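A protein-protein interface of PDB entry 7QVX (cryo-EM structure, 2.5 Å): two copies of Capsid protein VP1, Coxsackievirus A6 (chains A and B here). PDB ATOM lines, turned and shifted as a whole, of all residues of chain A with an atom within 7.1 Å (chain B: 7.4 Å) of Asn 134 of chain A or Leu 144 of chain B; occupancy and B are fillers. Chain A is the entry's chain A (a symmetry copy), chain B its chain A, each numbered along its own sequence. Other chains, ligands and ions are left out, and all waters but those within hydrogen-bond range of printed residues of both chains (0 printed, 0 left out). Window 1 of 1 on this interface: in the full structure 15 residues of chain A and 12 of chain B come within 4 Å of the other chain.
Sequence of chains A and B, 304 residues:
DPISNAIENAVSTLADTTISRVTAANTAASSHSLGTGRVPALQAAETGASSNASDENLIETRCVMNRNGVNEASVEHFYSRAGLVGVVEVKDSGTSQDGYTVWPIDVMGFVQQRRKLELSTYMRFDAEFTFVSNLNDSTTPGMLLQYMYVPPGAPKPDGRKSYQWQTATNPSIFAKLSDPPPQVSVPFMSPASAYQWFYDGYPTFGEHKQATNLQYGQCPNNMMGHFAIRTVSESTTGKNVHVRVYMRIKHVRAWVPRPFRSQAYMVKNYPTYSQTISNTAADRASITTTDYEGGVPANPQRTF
Positions printed for both chains: 141, 145, 147 and 177.
Of the 16 pairs that touch across the chains among the printed residues, none has its exchanged pair printed and touching as well.
Of chain B, only Leu 144 and Val 232 come within 4 Å of Asn 134 of chain A.
Of the printed residues of chain B, Ser 138 of chain A touches Gly 142, Met 143, Leu 144, Val 232 and Ser 233.
Printed residues of chain B within 4 Å of Arg 244 of chain A: Val 232 (3.3 Å).
Pro 141 of chain B touches none of the printed residues of chain A.
Leu 144 of chain B touches just these residues of chain A: Val 132, Asn 134 and Ser 138.
Ser 178 of chain B touches none of the printed residues of chain A.
The nearest printed residue of chain B that does not touch His 242 of chain A is Val 232 of chain B (6.7 Å).
Val 132 of chain A touches Phe 174 of chain B (CG1 to CD1, 3.95 Å).
ND2 of Asn 134 of chain A touches CD2 of Leu 144 of chain B, at 3.8 Å.
Asn 136 of chain A touches Ser 233 of chain B (O to CA, 3.5 Å).
Ser 138 of chain A touches Gly 142 of chain B (O to O, 3.6 Å).
Met 143 of chain B touches Ser 138 of chain A (CA to O, 3.4 Å).
Ser 138 of chain A touches Val 232 of chain B (CB to O, 3.1 Å).
CB of Ser 233 of chain B touches CB of Ser 138 of chain A, 3.9 Å away.
OG1 of Thr 140 of chain A touches CD of Lys 176 of chain B, 3.1 Å away.
His 242 of chain A touches Glu 234 of chain B.
NH1 of Arg 244 of chain A touches CG1 of Val 232 of chain B, at 3.3 Å.
Hydrophobic or aromatic side chains of chain A that line the printed part of chain B: Val 132 and His 242.
Along chain A the printed residues that touch a printed residue of chain B span positions 132 to 244.
Of the 19 printed residues of chain B, 8 touch a printed residue of chain A.
Hydrophobic or aromatic side chains of chain B that line the printed part of chain A: Met 143, Leu 144, Phe 174 and Val 232.
Among the printed residues, 16 pairs touch across the chains.
N of Val 232 of chain B lies within hydrogen-bond range of O of Leu 144 of chain B (3.0 Å).
The side-chain carboxylate (OD2) of Asp 179 of chain B is in salt-bridge range of the side-chain amino group (NZ) of Lys 176 of chain B, at 3.4 Å.
The side-chain hydroxyl of Thr 231 of chain B sits at hydrogen-bond distance from the side-chain hydroxyl of Ser 233 of chain B.
N of His 242 of chain A is in hydrogen-bond range of O of Asn 134 of chain A, 2.9 Å away.
The backbone NH of Leu 177 of chain B is in hydrogen-bond range of the backbone carbonyl oxygen of Met 143 of chain B (2.9 Å).
N of Thr 140 of chain A lies within hydrogen-bond range of O of Gly 142 of chain B, 3.2 Å away.
ND2 of Asn 134 of chain A sits at hydrogen-bond distance from O of Val 232 of chain B (2.6 Å).
N of Leu 144 of chain B lies within hydrogen-bond range of O of Ser 138 of chain A (2.9 Å).
N of Glu 234 of chain B lies within hydrogen-bond range of O of Asn 136 of chain A (3.0 Å).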
ATOM      1  N   VAL A 132      -5.619  16.925 -29.588  1.00  0.00           N
ATOM      2  CA  VAL A 132      -5.186  16.596 -28.209  1.00  0.00           C
ATOM      3  C   VAL A 132      -5.477  15.125 -28.010  1.00  0.00           C
ATOM      4  O   VAL A 132      -6.634  14.751 -27.923  1.00  0.00           O
ATOM      5  CB  VAL A 132      -5.869  17.486 -27.163  1.00  0.00           C
ATOM      6  CG1 VAL A 132      -5.430  17.118 -25.759  1.00  0.00           C
ATOM      7  CG2 VAL A 132      -5.587  18.951 -27.430  1.00  0.00           C
ATOM      8  N   SER A 133      -4.437  14.314 -27.925  1.00  0.00           N
ATOM      9  CA  SER A 133      -4.557  12.840 -27.967  1.00  0.00           C
ATOM     10  C   SER A 133      -3.939  12.240 -26.718  1.00  0.00           C
ATOM     11  O   SER A 133      -2.853  12.701 -26.295  1.00  0.00           O
ATOM     12  CB  SER A 133      -3.923  12.287 -29.204  1.00  0.00           C
ATOM     13  OG  SER A 133      -4.350  13.002 -30.356  1.00  0.00           O
ATOM     14  N   ASN A 134      -4.579  11.212 -26.183  1.00  0.00           N
ATOM     15  CA  ASN A 134      -4.036  10.450 -25.038  1.00  0.00           C
ATOM     16  C   ASN A 134      -4.748   9.109 -24.993  1.00  0.00           C
ATOM     17  O   ASN A 134      -5.631   8.866 -25.822  1.00  0.00           O
ATOM     18  CB  ASN A 134      -4.170  11.261 -23.745  1.00  0.00           C
ATOM     19  CG  ASN A 134      -5.607  11.581 -23.396  1.00  0.00           C
ATOM     20  OD1 ASN A 134      -6.487  11.585 -24.246  1.00  0.00           O
ATOM     21  ND2 ASN A 134      -5.869  11.875 -22.147  1.00  0.00           N
ATOM     22  N   LEU A 135      -4.397   8.273 -24.029  1.00  0.00           N
ATOM     23  CA  LEU A 135      -5.051   6.958 -23.848  1.00  0.00           C
ATOM     24  C   LEU A 135      -6.206   7.093 -22.856  1.00  0.00           C
ATOM     25  O   LEU A 135      -6.536   8.213 -22.456  1.00  0.00           O
ATOM     26  CB  LEU A 135      -4.002   5.951 -23.380  1.00  0.00           C
ATOM     27  CG  LEU A 135      -2.871   5.643 -24.356  1.00  0.00           C
ATOM     28  CD1 LEU A 135      -1.899   4.669 -23.707  1.00  0.00           C
ATOM     29  CD2 LEU A 135      -3.394   5.064 -25.674  1.00  0.00           C
ATOM     30  N   ASN A 136      -6.843   5.984 -22.497  1.00  0.00           N
ATOM     31  CA  ASN A 136      -8.002   5.976 -21.567  1.00  0.00           C
ATOM     32  C   ASN A 136      -7.620   6.578 -20.213  1.00  0.00           C
ATOM     33  O   ASN A 136      -8.410   7.369 -19.679  1.00  0.00           O
ATOM     34  CB  ASN A 136      -8.561   4.565 -21.378  1.00  0.00           C
ATOM     35  CG  ASN A 136      -9.420   4.126 -22.548  1.00  0.00           C
ATOM     36  OD1 ASN A 136      -9.923   4.954 -23.305  1.00  0.00           O
ATOM     37  ND2 ASN A 136      -9.595   2.822 -22.702  1.00  0.00           N
ATOM     38  N   ASP A 137      -6.447   6.236 -19.687  1.00  0.00           N
ATOM     39  CA  ASP A 137      -6.014   6.643 -18.323  1.00  0.00           C
ATOM     40  C   ASP A 137      -5.199   7.946 -18.359  1.00  0.00           C
ATOM     41  O   ASP A 137      -4.381   8.146 -17.450  1.00  0.00           O
ATOM     42  CB  ASP A 137      -5.224   5.499 -17.700  1.00  0.00           C
ATOM     43  CG  ASP A 137      -3.990   5.098 -18.501  1.00  0.00           C
ATOM     44  OD1 ASP A 137      -3.811   5.628 -19.625  1.00  0.00           O
ATOM     45  OD2 ASP A 137      -3.223   4.245 -18.005  1.00  0.00           O
ATOM     46  N   SER A 138      -5.373   8.785 -19.382  1.00  0.00           N
ATOM     47  CA  SER A 138      -4.700  10.098 -19.578  1.00  0.00           C
ATOM     48  C   SER A 138      -3.207   9.957 -19.897  1.00  0.00           C
ATOM     49  O   SER A 138      -2.575  11.004 -20.101  1.00  0.00           O
ATOM     50  CB  SER A 138      -4.910  11.028 -18.405  1.00  0.00           C
ATOM     51  OG  SER A 138      -4.233  10.579 -17.244  1.00  0.00           O
ATOM     52  N   THR A 139      -2.652   8.755 -19.984  1.00  0.00           N
ATOM     53  CA  THR A 139      -1.207   8.586 -20.275  1.00  0.00           C
ATOM     54  C   THR A 139      -0.929   8.947 -21.733  1.00  0.00           C
ATOM     55  O   THR A 139      -1.810   8.790 -22.590  1.00  0.00           O
ATOM     56  CB  THR A 139      -0.738   7.172 -19.943  1.00  0.00           C
ATOM     57  OG1 THR A 139      -1.502   6.250 -20.722  1.00  0.00           O
ATOM     58  CG2 THR A 139      -0.902   6.871 -18.472  1.00  0.00           C
ATOM     59  N   THR A 140       0.270   9.435 -22.007  1.00  0.00           N
ATOM     60  CA  THR A 140       0.711   9.784 -23.377  1.00  0.00           C
ATOM     61  C   THR A 140       2.059   9.120 -23.636  1.00  0.00           C
ATOM     62  O   THR A 140       3.073   9.812 -23.564  1.00  0.00           O
ATOM     63  CB  THR A 140       0.827  11.308 -23.554  1.00  0.00           C
ATOM     64  OG1 THR A 140       1.561  11.832 -22.448  1.00  0.00           O
ATOM     65  CG2 THR A 140      -0.497  12.035 -23.642  1.00  0.00           C
ATOM     66  N   PRO A 141       2.157   7.790 -23.926  1.00  0.00           N
ATOM     67  CA  PRO A 141       3.455   7.168 -24.212  1.00  0.00           C
ATOM     68  C   PRO A 141       3.965   7.538 -25.613  1.00  0.00           C
ATOM     69  O   PRO A 141       3.397   8.396 -26.250  1.00  0.00           O
ATOM     70  CB  PRO A 141       3.149   5.672 -24.092  1.00  0.00           C
ATOM     71  CG  PRO A 141       1.734   5.572 -24.578  1.00  0.00           C
ATOM     72  CD  PRO A 141       1.059   6.807 -24.009  1.00  0.00           C
ATOM     73  N   LEU A 145       1.422   8.348 -34.251  1.00  0.00           N
ATOM     74  CA  LEU A 145       0.087   8.493 -34.867  1.00  0.00           C
ATOM     75  C   LEU A 145       0.227   9.231 -36.186  1.00  0.00           C
ATOM     76  O   LEU A 145       1.125  10.086 -36.338  1.00  0.00           O
ATOM     77  CB  LEU A 145      -0.847   9.257 -33.928  1.00  0.00           C
ATOM     78  CG  LEU A 145      -1.831   8.403 -33.133  1.00  0.00           C
ATOM     79  CD1 LEU A 145      -1.149   7.744 -31.944  1.00  0.00           C
ATOM     80  CD2 LEU A 145      -3.002   9.256 -32.665  1.00  0.00           C
ATOM     81  N   TYR A 147      -2.033  11.646 -38.699  1.00  0.00           N
ATOM     82  CA  TYR A 147      -3.235  12.480 -38.887  1.00  0.00           C
ATOM     83  C   TYR A 147      -3.276  12.862 -40.350  1.00  0.00           C
ATOM     84  O   TYR A 147      -2.503  13.741 -40.774  1.00  0.00           O
ATOM     85  CB  TYR A 147      -3.163  13.725 -38.016  1.00  0.00           C
ATOM     86  CG  TYR A 147      -3.001  13.447 -36.549  1.00  0.00           C
ATOM     87  CD1 TYR A 147      -1.743  13.283 -35.998  1.00  0.00           C
ATOM     88  CD2 TYR A 147      -4.097  13.386 -35.712  1.00  0.00           C
ATOM     89  CE1 TYR A 147      -1.576  13.047 -34.647  1.00  0.00           C
ATOM     90  CE2 TYR A 147      -3.950  13.128 -34.363  1.00  0.00           C
ATOM     91  CZ  TYR A 147      -2.684  12.980 -33.830  1.00  0.00           C
ATOM     92  OH  TYR A 147      -2.531  12.770 -32.496  1.00  0.00           O
ATOM     93  N   LEU A 177       2.297  10.580 -29.267  1.00  0.00           N
ATOM     94  CA  LEU A 177       1.403  10.979 -28.156  1.00  0.00           C
ATOM     95  C   LEU A 177       2.183  11.788 -27.122  1.00  0.00           C
ATOM     96  O   LEU A 177       1.554  12.647 -26.478  1.00  0.00           O
ATOM     97  CB  LEU A 177       0.785   9.745 -27.499  1.00  0.00           C
ATOM     98  CG  LEU A 177      -0.260   8.992 -28.310  1.00  0.00           C
ATOM     99  CD1 LEU A 177      -0.972   7.983 -27.425  1.00  0.00           C
ATOM    100  CD2 LEU A 177      -1.265   9.949 -28.931  1.00  0.00           C
ATOM    101  N   PRO A 181       0.590  18.855 -28.701  1.00  0.00           N
ATOM    102  CA  PRO A 181      -0.468  18.543 -29.666  1.00  0.00           C
ATOM    103  C   PRO A 181      -0.153  19.039 -31.072  1.00  0.00           C
ATOM    104  O   PRO A 181       0.333  20.157 -31.241  1.00  0.00           O
ATOM    105  CB  PRO A 181      -1.681  19.294 -29.114  1.00  0.00           C
ATOM    106  CG  PRO A 181      -1.389  19.416 -27.638  1.00  0.00           C
ATOM    107  CD  PRO A 181       0.098  19.673 -27.577  1.00  0.00           C
ATOM    108  N   ASN A 240      -6.817   1.955 -26.924  1.00  0.00           N
ATOM    109  CA  ASN A 240      -7.714   2.961 -27.533  1.00  0.00           C
ATOM    110  C   ASN A 240      -7.098   4.345 -27.363  1.00  0.00           C
ATOM    111  O   ASN A 240      -6.651   4.679 -26.261  1.00  0.00           O
ATOM    112  CB  ASN A 240      -9.114   2.882 -26.937  1.00  0.00           C
ATOM    113  CG  ASN A 240      -9.825   1.595 -27.290  1.00  0.00           C
ATOM    114  OD1 ASN A 240      -9.309   0.769 -28.043  1.00  0.00           O
ATOM    115  ND2 ASN A 240     -11.023   1.420 -26.766  1.00  0.00           N
ATOM    116  N   VAL A 241      -7.111   5.132 -28.428  1.00  0.00           N
ATOM    117  CA  VAL A 241      -6.603   6.525 -28.407  1.00  0.00           C
ATOM    118  C   VAL A 241      -7.790   7.470 -28.545  1.00  0.00           C
ATOM    119  O   VAL A 241      -8.535   7.381 -29.534  1.00  0.00           O
ATOM    120  CB  VAL A 241      -5.560   6.750 -29.504  1.00  0.00           C
ATOM    121  CG1 VAL A 241      -5.018   8.164 -29.452  1.00  0.00           C
ATOM    122  CG2 VAL A 241      -4.436   5.736 -29.399  1.00  0.00           C
ATOM    123  N   HIS A 242      -7.940   8.370 -27.586  1.00  0.00           N
ATOM    124  CA  HIS A 242      -8.956   9.446 -27.633  1.00  0.00           C
ATOM    125  C   HIS A 242      -8.318  10.689 -28.222  1.00  0.00           C
ATOM    126  O   HIS A 242      -7.323  11.178 -27.659  1.00  0.00           O
ATOM    127  CB  HIS A 242      -9.527   9.715 -26.245  1.00  0.00           C
ATOM    128  CG  HIS A 242     -10.327   8.577 -25.716  1.00  0.00           C
ATOM    129  ND1 HIS A 242     -11.711   8.524 -25.838  1.00  0.00           N
ATOM    130  CD2 HIS A 242      -9.948   7.431 -25.102  1.00  0.00           C
ATOM    131  CE1 HIS A 242     -12.145   7.396 -25.300  1.00  0.00           C
ATOM    132  NE2 HIS A 242     -11.079   6.698 -24.858  1.00  0.00           N
ATOM    133  N   VAL A 243      -8.869  11.193 -29.312  1.00  0.00           N
ATOM    134  CA  VAL A 243      -8.350  12.422 -29.962  1.00  0.00           C
ATOM    135  C   VAL A 243      -9.402  13.504 -29.780  1.00  0.00           C
ATOM    136  O   VAL A 243     -10.506  13.359 -30.310  1.00  0.00           O
ATOM    137  CB  VAL A 243      -8.011  12.187 -31.441  1.00  0.00           C
ATOM    138  CG1 VAL A 243      -7.556  13.479 -32.105  1.00  0.00           C
ATOM    139  CG2 VAL A 243      -6.960  11.101 -31.588  1.00  0.00           C
ATOM    140  N   ARG A 244      -9.043  14.566 -29.082  1.00  0.00           N
ATOM    141  CA  ARG A 244      -9.893  15.759 -28.944  1.00  0.00           C
ATOM    142  C   ARG A 244      -9.494  16.755 -30.023  1.00  0.00           C
ATOM    143  O   ARG A 244      -8.365  17.270 -30.005  1.00  0.00           O
ATOM    144  CB  ARG A 244      -9.752  16.374 -27.559  1.00  0.00           C
ATOM    145  CG  ARG A 244     -10.527  15.618 -26.502  1.00  0.00           C
ATOM    146  CD  ARG A 244     -10.296  16.201 -25.119  1.00  0.00           C
ATOM    147  NE  ARG A 244     -11.260  15.625 -24.187  1.00  0.00           N
ATOM    148  CZ  ARG A 244     -11.286  14.343 -23.781  1.00  0.00           C
ATOM    149  NH1 ARG A 244     -10.392  13.451 -24.202  1.00  0.00           N
ATOM    150  NH2 ARG A 244     -12.226  13.957 -22.930  1.00  0.00           N
ATOM    151  N   PRO B 141       4.845  11.623 -14.645  1.00  0.00           N
ATOM    152  CA  PRO B 141       4.731  10.843 -15.883  1.00  0.00           C
ATOM    153  C   PRO B 141       3.982  11.619 -16.975  1.00  0.00           C
ATOM    154  O   PRO B 141       3.729  12.791 -16.810  1.00  0.00           O
ATOM    155  CB  PRO B 141       3.958   9.600 -15.432  1.00  0.00           C
ATOM    156  CG  PRO B 141       3.051  10.131 -14.361  1.00  0.00           C
ATOM    157  CD  PRO B 141       3.911  11.134 -13.612  1.00  0.00           C
ATOM    158  N   GLY B 142       3.628  10.963 -18.074  1.00  0.00           N
ATOM    159  CA  GLY B 142       3.026  11.656 -19.224  1.00  0.00           C
ATOM    160  C   GLY B 142       1.531  11.854 -19.099  1.00  0.00           C
ATOM    161  O   GLY B 142       0.896  11.937 -20.148  1.00  0.00           O
ATOM    162  N   MET B 143       0.976  11.945 -17.895  1.00  0.00           N
ATOM    163  CA  MET B 143      -0.477  12.168 -17.723  1.00  0.00           C
ATOM    164  C   MET B 143      -0.852  13.535 -18.298  1.00  0.00           C
ATOM    165  O   MET B 143      -0.138  14.521 -18.067  1.00  0.00           O
ATOM    166  CB  MET B 143      -0.873  12.105 -16.252  1.00  0.00           C
ATOM    167  CG  MET B 143      -0.714  10.716 -15.670  1.00  0.00           C
ATOM    168  SD  MET B 143      -1.166  10.660 -13.920  1.00  0.00           S
ATOM    169  CE  MET B 143      -2.944  10.835 -14.037  1.00  0.00           C
ATOM    170  N   LEU B 144      -1.944  13.587 -19.041  1.00  0.00           N
ATOM    171  CA  LEU B 144      -2.444  14.841 -19.646  1.00  0.00           C
ATOM    172  C   LEU B 144      -3.450  15.488 -18.699  1.00  0.00           C
ATOM    173  O   LEU B 144      -4.360  14.805 -18.189  1.00  0.00           O
ATOM    174  CB  LEU B 144      -3.079  14.537 -20.996  1.00  0.00           C
ATOM    175  CG  LEU B 144      -3.659  15.738 -21.734  1.00  0.00           C
ATOM    176  CD1 LEU B 144      -2.585  16.746 -22.098  1.00  0.00           C
ATOM    177  CD2 LEU B 144      -4.384  15.286 -22.985  1.00  0.00           C
ATOM    178  N   LEU B 145      -3.288  16.781 -18.482  1.00  0.00           N
ATOM    179  CA  LEU B 145      -4.145  17.554 -17.559  1.00  0.00           C
ATOM    180  C   LEU B 145      -4.764  18.716 -18.314  1.00  0.00           C
ATOM    181  O   LEU B 145      -4.148  19.255 -19.258  1.00  0.00           O
ATOM    182  CB  LEU B 145      -3.321  18.068 -16.379  1.00  0.00           C
ATOM    183  CG  LEU B 145      -3.456  17.276 -15.081  1.00  0.00           C
ATOM    184  CD1 LEU B 145      -2.625  16.003 -15.127  1.00  0.00           C
ATOM    185  CD2 LEU B 145      -3.037  18.138 -13.898  1.00  0.00           C
ATOM    186  N   GLN B 146      -5.961  19.098 -17.894  1.00  0.00           N
ATOM    187  CA  GLN B 146      -6.640  20.288 -18.442  1.00  0.00           C
ATOM    188  C   GLN B 146      -6.770  21.321 -17.328  1.00  0.00           C
ATOM    189  O   GLN B 146      -7.354  21.027 -16.292  1.00  0.00           O
ATOM    190  CB  GLN B 146      -7.994  19.904 -19.019  1.00  0.00           C
ATOM    191  CG  GLN B 146      -8.690  21.078 -19.688  1.00  0.00           C
ATOM    192  CD  GLN B 146     -10.069  20.726 -20.176  1.00  0.00           C
ATOM    193  OE1 GLN B 146     -10.546  19.606 -20.000  1.00  0.00           O
ATOM    194  NE2 GLN B 146     -10.723  21.687 -20.797  1.00  0.00           N
ATOM    195  N   TYR B 147      -6.268  22.515 -17.568  1.00  0.00           N
ATOM    196  CA  TYR B 147      -6.388  23.653 -16.639  1.00  0.00           C
ATOM    197  C   TYR B 147      -7.364  24.626 -17.265  1.00  0.00           C
ATOM    198  O   TYR B 147      -6.992  25.339 -18.215  1.00  0.00           O
ATOM    199  CB  TYR B 147      -5.036  24.320 -16.431  1.00  0.00           C
ATOM    200  CG  TYR B 147      -3.964  23.402 -15.922  1.00  0.00           C
ATOM    201  CD1 TYR B 147      -3.194  22.662 -16.802  1.00  0.00           C
ATOM    202  CD2 TYR B 147      -3.696  23.302 -14.571  1.00  0.00           C
ATOM    203  CE1 TYR B 147      -2.189  21.827 -16.350  1.00  0.00           C
ATOM    204  CE2 TYR B 147      -2.711  22.454 -14.100  1.00  0.00           C
ATOM    205  CZ  TYR B 147      -1.945  21.734 -14.996  1.00  0.00           C
ATOM    206  OH  TYR B 147      -0.946  20.932 -14.541  1.00  0.00           O
ATOM    207  N   ILE B 173      -5.866  25.142 -20.655  1.00  0.00           N
ATOM    208  CA  ILE B 173      -4.479  24.735 -20.953  1.00  0.00           C
ATOM    209  C   ILE B 173      -4.455  23.220 -20.904  1.00  0.00           C
ATOM    210  O   ILE B 173      -4.793  22.643 -19.875  1.00  0.00           O
ATOM    211  CB  ILE B 173      -3.491  25.373 -19.977  1.00  0.00           C
ATOM    212  CG1 ILE B 173      -3.609  26.893 -20.009  1.00  0.00           C
ATOM    213  CG2 ILE B 173      -2.077  24.921 -20.308  1.00  0.00           C
ATOM    214  CD1 ILE B 173      -2.739  27.594 -18.972  1.00  0.00           C
ATOM    215  N   PHE B 174      -3.998  22.609 -21.987  1.00  0.00           N
ATOM    216  CA  PHE B 174      -3.699  21.162 -22.026  1.00  0.00           C
ATOM    217  C   PHE B 174      -2.193  21.013 -21.917  1.00  0.00           C
ATOM    218  O   PHE B 174      -1.437  21.495 -22.797  1.00  0.00           O
ATOM    219  CB  PHE B 174      -4.286  20.535 -23.282  1.00  0.00           C
ATOM    220  CG  PHE B 174      -5.783  20.483 -23.266  1.00  0.00           C
ATOM    221  CD1 PHE B 174      -6.440  19.408 -22.702  1.00  0.00           C
ATOM    222  CD2 PHE B 174      -6.529  21.495 -23.855  1.00  0.00           C
ATOM    223  CE1 PHE B 174      -7.823  19.354 -22.713  1.00  0.00           C
ATOM    224  CE2 PHE B 174      -7.913  21.446 -23.850  1.00  0.00           C
ATOM    225  CZ  PHE B 174      -8.550  20.373 -23.277  1.00  0.00           C
ATOM    226  N   ALA B 175      -1.750  20.405 -20.835  1.00  0.00           N
ATOM    227  CA  ALA B 175      -0.314  20.182 -20.582  1.00  0.00           C
ATOM    228  C   ALA B 175      -0.135  18.826 -19.933  1.00  0.00           C
ATOM    229  O   ALA B 175      -1.005  18.373 -19.188  1.00  0.00           O
ATOM    230  CB  ALA B 175       0.250  21.276 -19.719  1.00  0.00           C
ATOM    231  N   LYS B 176       1.012  18.216 -20.179  1.00  0.00           N
ATOM    232  CA  LYS B 176       1.390  16.936 -19.545  1.00  0.00           C
ATOM    233  C   LYS B 176       2.151  17.210 -18.253  1.00  0.00           C
ATOM    234  O   LYS B 176       2.802  18.265 -18.147  1.00  0.00           O
ATOM    235  CB  LYS B 176       2.197  16.117 -20.538  1.00  0.00           C
ATOM    236  CG  LYS B 176       1.378  15.659 -21.731  1.00  0.00           C
ATOM    237  CD  LYS B 176       2.171  14.845 -22.727  1.00  0.00           C
ATOM    238  CE  LYS B 176       3.247  15.644 -23.431  1.00  0.00           C
ATOM    239  NZ  LYS B 176       2.663  16.682 -24.313  1.00  0.00           N
ATOM    240  N   LEU B 177       2.093  16.280 -17.306  1.00  0.00           N
ATOM    241  CA  LEU B 177       2.880  16.396 -16.056  1.00  0.00           C
ATOM    242  C   LEU B 177       4.372  16.416 -16.378  1.00  0.00           C
ATOM    243  O   LEU B 177       5.115  17.051 -15.607  1.00  0.00           O
ATOM    244  CB  LEU B 177       2.562  15.234 -15.115  1.00  0.00           C
ATOM    245  CG  LEU B 177       1.187  15.242 -14.463  1.00  0.00           C
ATOM    246  CD1 LEU B 177       1.134  14.200 -13.358  1.00  0.00           C
ATOM    247  CD2 LEU B 177       0.851  16.616 -13.907  1.00  0.00           C
ATOM    248  N   SER B 178       4.794  15.768 -17.461  1.00  0.00           N
ATOM    249  CA  SER B 178       6.215  15.705 -17.865  1.00  0.00           C
ATOM    250  C   SER B 178       6.658  17.017 -18.516  1.00  0.00           C
ATOM    251  O   SER B 178       7.873  17.183 -18.704  1.00  0.00           O
ATOM    252  CB  SER B 178       6.463  14.540 -18.769  1.00  0.00           C
ATOM    253  OG  SER B 178       5.724  14.677 -19.966  1.00  0.00           O
ATOM    254  N   ASP B 179       5.733  17.904 -18.869  1.00  0.00           N
ATOM    255  CA  ASP B 179       6.073  19.206 -19.493  1.00  0.00           C
ATOM    256  C   ASP B 179       6.541  20.178 -18.422  1.00  0.00           C
ATOM    257  O   ASP B 179       6.256  20.004 -17.244  1.00  0.00           O
ATOM    258  CB  ASP B 179       4.885  19.758 -20.274  1.00  0.00           C
ATOM    259  CG  ASP B 179       4.510  18.890 -21.483  1.00  0.00           C
ATOM    260  OD1 ASP B 179       5.364  18.055 -21.925  1.00  0.00           O
ATOM    261  OD2 ASP B 179       3.364  19.048 -21.996  1.00  0.00           O
ATOM    262  N   ARG B 230      -8.573  19.094 -14.127  1.00  0.00           N
ATOM    263  CA  ARG B 230      -8.900  17.655 -14.221  1.00  0.00           C
ATOM    264  C   ARG B 230      -7.813  16.933 -14.995  1.00  0.00           C
ATOM    265  O   ARG B 230      -7.068  17.571 -15.772  1.00  0.00           O
ATOM    266  CB  ARG B 230     -10.251  17.462 -14.900  1.00  0.00           C
ATOM    267  CG  ARG B 230     -10.249  17.778 -16.383  1.00  0.00           C
ATOM    268  CD  ARG B 230     -11.343  17.036 -17.094  1.00  0.00           C
ATOM    269  NE  ARG B 230     -11.412  17.428 -18.492  1.00  0.00           N
ATOM    270  CZ  ARG B 230     -12.251  16.906 -19.384  1.00  0.00           C
ATOM    271  NH1 ARG B 230     -13.122  15.973 -19.027  1.00  0.00           N
ATOM    272  NH2 ARG B 230     -12.227  17.331 -20.633  1.00  0.00           N
ATOM    273  N   THR B 231      -7.744  15.631 -14.808  1.00  0.00           N
ATOM    274  CA  THR B 231      -6.987  14.754 -15.723  1.00  0.00           C
ATOM    275  C   THR B 231      -7.888  14.430 -16.904  1.00  0.00           C
ATOM    276  O   THR B 231      -9.059  14.097 -16.696  1.00  0.00           O
ATOM    277  CB  THR B 231      -6.484  13.499 -15.021  1.00  0.00           C
ATOM    278  OG1 THR B 231      -7.613  12.797 -14.496  1.00  0.00           O
ATOM    279  CG2 THR B 231      -5.509  13.854 -13.924  1.00  0.00           C
ATOM    280  N   VAL B 232      -7.363  14.515 -18.109  1.00  0.00           N
ATOM    281  CA  VAL B 232      -8.175  14.205 -19.306  1.00  0.00           C
ATOM    282  C   VAL B 232      -8.209  12.686 -19.387  1.00  0.00           C
ATOM    283  O   VAL B 232      -7.316  12.117 -19.971  1.00  0.00           O
ATOM    284  CB  VAL B 232      -7.600  14.892 -20.549  1.00  0.00           C
ATOM    285  CG1 VAL B 232      -8.397  14.537 -21.795  1.00  0.00           C
ATOM    286  CG2 VAL B 232      -7.570  16.400 -20.354  1.00  0.00           C
ATOM    287  N   SER B 233      -9.158  12.055 -18.716  1.00  0.00           N
ATOM    288  CA  SER B 233      -9.251  10.574 -18.635  1.00  0.00           C
ATOM    289  C   SER B 233     -10.708  10.122 -18.645  1.00  0.00           C
ATOM    290  O   SER B 233     -11.576  10.917 -18.243  1.00  0.00           O
ATOM    291  CB  SER B 233      -8.560  10.064 -17.412  1.00  0.00           C
ATOM    292  OG  SER B 233      -9.225  10.516 -16.243  1.00  0.00           O
ATOM    293  N   GLU B 234     -10.953   8.875 -19.058  1.00  0.00           N
ATOM    294  CA  GLU B 234     -12.327   8.307 -19.153  1.00  0.00           C
ATOM    295  C   GLU B 234     -12.855   7.808 -17.806  1.00  0.00           C
ATOM    296  O   GLU B 234     -13.917   8.276 -17.372  1.00  0.00           O
ATOM    297  CB  GLU B 234     -12.380   7.154 -20.147  1.00  0.00           C
ATOM    298  CG  GLU B 234     -12.087   7.580 -21.567  1.00  0.00           C
ATOM    299  CD  GLU B 234     -12.901   8.766 -22.069  1.00  0.00           C
ATOM    300  OE1 GLU B 234     -14.129   8.608 -22.274  1.00  0.00           O
ATOM    301  OE2 GLU B 234     -12.312   9.855 -22.235  1.00  0.00           O
